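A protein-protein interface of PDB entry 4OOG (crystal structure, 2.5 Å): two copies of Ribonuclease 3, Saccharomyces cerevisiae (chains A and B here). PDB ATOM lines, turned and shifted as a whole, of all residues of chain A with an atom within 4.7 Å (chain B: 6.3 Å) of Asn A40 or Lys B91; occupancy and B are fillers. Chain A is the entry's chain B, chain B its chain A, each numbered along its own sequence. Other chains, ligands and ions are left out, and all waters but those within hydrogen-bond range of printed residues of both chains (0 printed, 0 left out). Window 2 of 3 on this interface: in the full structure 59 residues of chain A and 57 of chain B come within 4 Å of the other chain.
The backbone carbonyl oxygen of Gln B92 sits at hydrogen-bond distance from the side-chain amino group of Lys A59 (2.7 Å).
The backbone carbonyl oxygen (O) of Gln B90 sits at hydrogen-bond distance from the side-chain amino group (NZ) of Lys A59, at 3.1 Å.
The side-chain amide oxygen (OD1) of Asn A40 is in hydrogen-bond range of the side-chain amino group (NZ) of Lys B91, 3.1 Å away.
The backbone carbonyl oxygen of Asn A36 lies within hydrogen-bond range of the side-chain amide nitrogen of Asn A40, 2.6 Å away.
The side-chain carboxylate (OD2) of Asp B87 sits close to the side-chain amide nitrogen (NE2) of Gln B90, 3.4 Å away.
Of chain B, only Lys B91 comes within 4 Å of Asn A40.
Of the printed residues of chain A, Gln B90 touches Lys A59 (3.1 Å).
Lys B91 touches one residue of chain A.
Printed residues of chain A within 4 Å of Gln B92: Lys A59 (2.7 Å).
The nearest residue of chain A that does not touch Lys B91 is Lys A59 (4.2 Å).
The nearest printed residue of chain A that does not touch Gln B92 is Asn A36 (6.6 Å).
Printed residues of chain A that touch a printed residue of chain B: Asn A40 and Lys A59.
Among the printed residues, no Asp or Glu carboxylate lies within 4 Å of a Lys or Arg side-chain nitrogen of the other chain.
No position is printed for both chains.
Of the 3 pairs that touch across the chains among the printed residues, none has its exchanged pair printed and touching as well.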
ATOM      1  N   ASN A  36      19.271 -24.008 -10.977  1.00  0.00           N
ATOM      2  CA  ASN A  36      19.231 -23.130  -9.813  1.00  0.00           C
ATOM      3  C   ASN A  36      18.083 -23.459  -8.866  1.00  0.00           C
ATOM      4  O   ASN A  36      18.212 -23.310  -7.654  1.00  0.00           O
ATOM      5  CB  ASN A  36      19.172 -21.659 -10.238  1.00  0.00           C
ATOM      6  CG  ASN A  36      20.549 -21.065 -10.480  1.00  0.00           C
ATOM      7  OD1 ASN A  36      21.536 -21.488  -9.875  1.00  0.00           O
ATOM      8  ND2 ASN A  36      20.620 -20.072 -11.360  1.00  0.00           N
ATOM      9  N   GLU A  37      16.965 -23.917  -9.421  1.00  0.00           N
ATOM     10  CA  GLU A  37      15.832 -24.331  -8.603  1.00  0.00           C
ATOM     11  C   GLU A  37      16.168 -25.579  -7.792  1.00  0.00           C
ATOM     12  O   GLU A  37      15.941 -25.627  -6.583  1.00  0.00           O
ATOM     13  CB  GLU A  37      14.600 -24.605  -9.469  1.00  0.00           C
ATOM     14  CG  GLU A  37      13.370 -24.993  -8.661  1.00  0.00           C
ATOM     15  CD  GLU A  37      12.467 -25.974  -9.386  1.00  0.00           C
ATOM     16  OE1 GLU A  37      12.284 -25.831 -10.613  1.00  0.00           O
ATOM     17  OE2 GLU A  37      11.945 -26.896  -8.721  1.00  0.00           O
ATOM     18  N   ALA A  38      16.713 -26.585  -8.470  1.00  0.00           N
ATOM     19  CA  ALA A  38      17.031 -27.859  -7.837  1.00  0.00           C
ATOM     20  C   ALA A  38      18.120 -27.718  -6.781  1.00  0.00           C
ATOM     21  O   ALA A  38      18.024 -28.297  -5.697  1.00  0.00           O
ATOM     22  CB  ALA A  38      17.442 -28.878  -8.885  1.00  0.00           C
ATOM     23  N   VAL A  39      19.156 -26.951  -7.098  1.00  0.00           N
ATOM     24  CA  VAL A  39      20.284 -26.800  -6.187  1.00  0.00           C
ATOM     25  C   VAL A  39      19.887 -25.990  -4.952  1.00  0.00           C
ATOM     26  O   VAL A  39      20.439 -26.188  -3.871  1.00  0.00           O
ATOM     27  CB  VAL A  39      21.518 -26.179  -6.890  1.00  0.00           C
ATOM     28  CG1 VAL A  39      21.319 -24.689  -7.129  1.00  0.00           C
ATOM     29  CG2 VAL A  39      22.778 -26.433  -6.077  1.00  0.00           C
ATOM     30  N   ASN A  40      18.916 -25.094  -5.113  1.00  0.00           N
ATOM     31  CA  ASN A  40      18.441 -24.273  -4.003  1.00  0.00           C
ATOM     32  C   ASN A  40      17.504 -25.019  -3.058  1.00  0.00           C
ATOM     33  O   ASN A  40      17.664 -24.951  -1.840  1.00  0.00           O
ATOM     34  CB  ASN A  40      17.794 -22.982  -4.510  1.00  0.00           C
ATOM     35  CG  ASN A  40      18.817 -21.978  -5.011  1.00  0.00           C
ATOM     36  OD1 ASN A  40      19.917 -21.871  -4.465  1.00  0.00           O
ATOM     37  ND2 ASN A  40      18.464 -21.242  -6.058  1.00  0.00           N
ATOM     38  N   ASN A  41      16.528 -25.731  -3.613  1.00  0.00           N
ATOM     39  CA  ASN A  41      15.710 -26.605  -2.788  1.00  0.00           C
ATOM     40  C   ASN A  41      16.076 -28.039  -3.102  1.00  0.00           C
ATOM     41  O   ASN A  41      15.667 -28.585  -4.124  1.00  0.00           O
ATOM     42  CB  ASN A  41      14.229 -26.391  -3.091  1.00  0.00           C
ATOM     43  CG  ASN A  41      13.921 -24.969  -3.511  1.00  0.00           C
ATOM     44  OD1 ASN A  41      14.553 -24.022  -3.045  1.00  0.00           O
ATOM     45  ND2 ASN A  41      12.950 -24.815  -4.402  1.00  0.00           N
ATOM     46  N   GLN A  42      16.835 -28.652  -2.201  1.00  0.00           N
ATOM     47  CA  GLN A  42      17.301 -30.015  -2.393  1.00  0.00           C
ATOM     48  C   GLN A  42      16.465 -31.015  -1.610  1.00  0.00           C
ATOM     49  O   GLN A  42      16.691 -32.222  -1.676  1.00  0.00           O
ATOM     50  CB  GLN A  42      18.782 -30.121  -2.036  1.00  0.00           C
ATOM     51  CG  GLN A  42      19.658 -29.233  -2.901  1.00  0.00           C
ATOM     52  CD  GLN A  42      21.129 -29.478  -2.675  1.00  0.00           C
ATOM     53  OE1 GLN A  42      21.510 -30.263  -1.809  1.00  0.00           O
ATOM     54  NE2 GLN A  42      21.968 -28.808  -3.457  1.00  0.00           N
ATOM     55  N   LYS A  59      26.143 -28.159 -13.469  1.00  0.00           N
ATOM     56  CA  LYS A  59      26.089 -26.718 -13.660  1.00  0.00           C
ATOM     57  C   LYS A  59      26.627 -26.373 -15.044  1.00  0.00           C
ATOM     58  O   LYS A  59      26.036 -25.576 -15.770  1.00  0.00           O
ATOM     59  CB  LYS A  59      26.895 -25.998 -12.580  1.00  0.00           C
ATOM     60  CG  LYS A  59      26.589 -24.514 -12.471  1.00  0.00           C
ATOM     61  CD  LYS A  59      27.442 -23.853 -11.403  1.00  0.00           C
ATOM     62  CE  LYS A  59      27.136 -22.371 -11.291  1.00  0.00           C
ATOM     63  NZ  LYS A  59      27.975 -21.717 -10.248  1.00  0.00           N
ATOM     64  N   ASP B  87      32.353 -23.541  -7.690  1.00  0.00           N
ATOM     65  CA  ASP B  87      32.228 -23.629  -6.245  1.00  0.00           C
ATOM     66  C   ASP B  87      30.764 -23.824  -5.868  1.00  0.00           C
ATOM     67  O   ASP B  87      29.868 -23.290  -6.523  1.00  0.00           O
ATOM     68  CB  ASP B  87      32.782 -22.373  -5.576  1.00  0.00           C
ATOM     69  CG  ASP B  87      32.834 -22.497  -4.068  1.00  0.00           C
ATOM     70  OD1 ASP B  87      33.419 -23.484  -3.574  1.00  0.00           O
ATOM     71  OD2 ASP B  87      32.278 -21.618  -3.377  1.00  0.00           O
ATOM     72  N   THR B  88      30.531 -24.591  -4.808  1.00  0.00           N
ATOM     73  CA  THR B  88      29.177 -24.953  -4.397  1.00  0.00           C
ATOM     74  C   THR B  88      28.304 -23.748  -4.052  1.00  0.00           C
ATOM     75  O   THR B  88      27.234 -23.564  -4.633  1.00  0.00           O
ATOM     76  CB  THR B  88      29.195 -25.910  -3.188  1.00  0.00           C
ATOM     77  OG1 THR B  88      29.856 -27.129  -3.548  1.00  0.00           O
ATOM     78  CG2 THR B  88      27.777 -26.220  -2.735  1.00  0.00           C
ATOM     79  N   GLU B  89      28.764 -22.929  -3.112  1.00  0.00           N
ATOM     80  CA  GLU B  89      27.960 -21.818  -2.608  1.00  0.00           C
ATOM     81  C   GLU B  89      27.962 -20.584  -3.507  1.00  0.00           C
ATOM     82  O   GLU B  89      27.193 -19.649  -3.282  1.00  0.00           O
ATOM     83  CB  GLU B  89      28.387 -21.434  -1.189  1.00  0.00           C
ATOM     84  CG  GLU B  89      29.880 -21.522  -0.941  1.00  0.00           C
ATOM     85  CD  GLU B  89      30.276 -22.827  -0.282  1.00  0.00           C
ATOM     86  OE1 GLU B  89      29.704 -23.153   0.780  1.00  0.00           O
ATOM     87  OE2 GLU B  89      31.154 -23.530  -0.827  1.00  0.00           O
ATOM     88  N   GLN B  90      28.818 -20.573  -4.524  1.00  0.00           N
ATOM     89  CA  GLN B  90      28.819 -19.469  -5.474  1.00  0.00           C
ATOM     90  C   GLN B  90      27.774 -19.744  -6.549  1.00  0.00           C
ATOM     91  O   GLN B  90      27.887 -20.707  -7.307  1.00  0.00           O
ATOM     92  CB  GLN B  90      30.203 -19.292  -6.100  1.00  0.00           C
ATOM     93  CG  GLN B  90      31.309 -19.013  -5.090  1.00  0.00           C
ATOM     94  CD  GLN B  90      32.662 -18.807  -5.745  1.00  0.00           C
ATOM     95  OE1 GLN B  90      32.751 -18.547  -6.945  1.00  0.00           O
ATOM     96  NE2 GLN B  90      33.727 -18.926  -4.959  1.00  0.00           N
ATOM     97  N   LYS B  91      26.760 -18.887  -6.611  1.00  0.00           N
ATOM     98  CA  LYS B  91      25.610 -19.116  -7.479  1.00  0.00           C
ATOM     99  C   LYS B  91      25.749 -18.409  -8.822  1.00  0.00           C
ATOM    100  O   LYS B  91      24.835 -18.434  -9.647  1.00  0.00           O
ATOM    101  CB  LYS B  91      24.318 -18.694  -6.775  1.00  0.00           C
ATOM    102  CG  LYS B  91      24.106 -19.378  -5.432  1.00  0.00           C
ATOM    103  CD  LYS B  91      24.137 -20.891  -5.581  1.00  0.00           C
ATOM    104  CE  LYS B  91      24.078 -21.590  -4.231  1.00  0.00           C
ATOM    105  NZ  LYS B  91      22.805 -21.314  -3.514  1.00  0.00           N
ATOM    106  N   GLN B  92      26.897 -17.773  -9.028  1.00  0.00           N
ATOM    107  CA  GLN B  92      27.192 -17.096 -10.285  1.00  0.00           C
ATOM    108  C   GLN B  92      27.364 -18.107 -11.414  1.00  0.00           C
ATOM    109  O   GLN B  92      27.883 -19.200 -11.196  1.00  0.00           O
ATOM    110  CB  GLN B  92      28.463 -16.261 -10.144  1.00  0.00           C
ATOM    111  CG  GLN B  92      28.435 -15.273  -8.993  1.00  0.00           C
ATOM    112  CD  GLN B  92      29.769 -14.585  -8.792  1.00  0.00           C
ATOM    113  OE1 GLN B  92      30.753 -14.908  -9.461  1.00  0.00           O
ATOM    114  NE2 GLN B  92      29.812 -13.632  -7.869  1.00  0.00           N
ATOM    115  N   PRO B  93      26.920 -17.745 -12.628  1.00  0.00           N
ATOM    116  CA  PRO B  93      27.037 -18.602 -13.814  1.00  0.00           C
ATOM    117  C   PRO B  93      28.478 -18.809 -14.286  1.00  0.00           C
ATOM    118  O   PRO B  93      28.760 -19.817 -14.927  1.00  0.00           O
ATOM    119  CB  PRO B  93      26.239 -17.838 -14.878  1.00  0.00           C
ATOM    120  CG  PRO B  93      25.310 -16.965 -14.103  1.00  0.00           C
ATOM    121  CD  PRO B  93      26.088 -16.559 -12.892  1.00  0.00           C
ATOM    122  N   ILE B  94      29.360 -17.855 -13.992  1.00  0.00           N
ATOM    123  CA  ILE B  94      30.796 -17.933 -14.318  1.00  0.00           C
ATOM    124  C   ILE B  94      31.167 -17.938 -15.814  1.00  0.00           C
ATOM    125  O   ILE B  94      32.351 -17.908 -16.158  1.00  0.00           O
ATOM    126  CB  ILE B  94      31.566 -19.065 -13.548  1.00  0.00           C
ATOM    127  CG1 ILE B  94      31.658 -20.351 -14.373  1.00  0.00           C
ATOM    128  CG2 ILE B  94      30.972 -19.298 -12.158  1.00  0.00           C
ATOM    129  CD1 ILE B  94      33.029 -20.989 -14.349  1.00  0.00           C
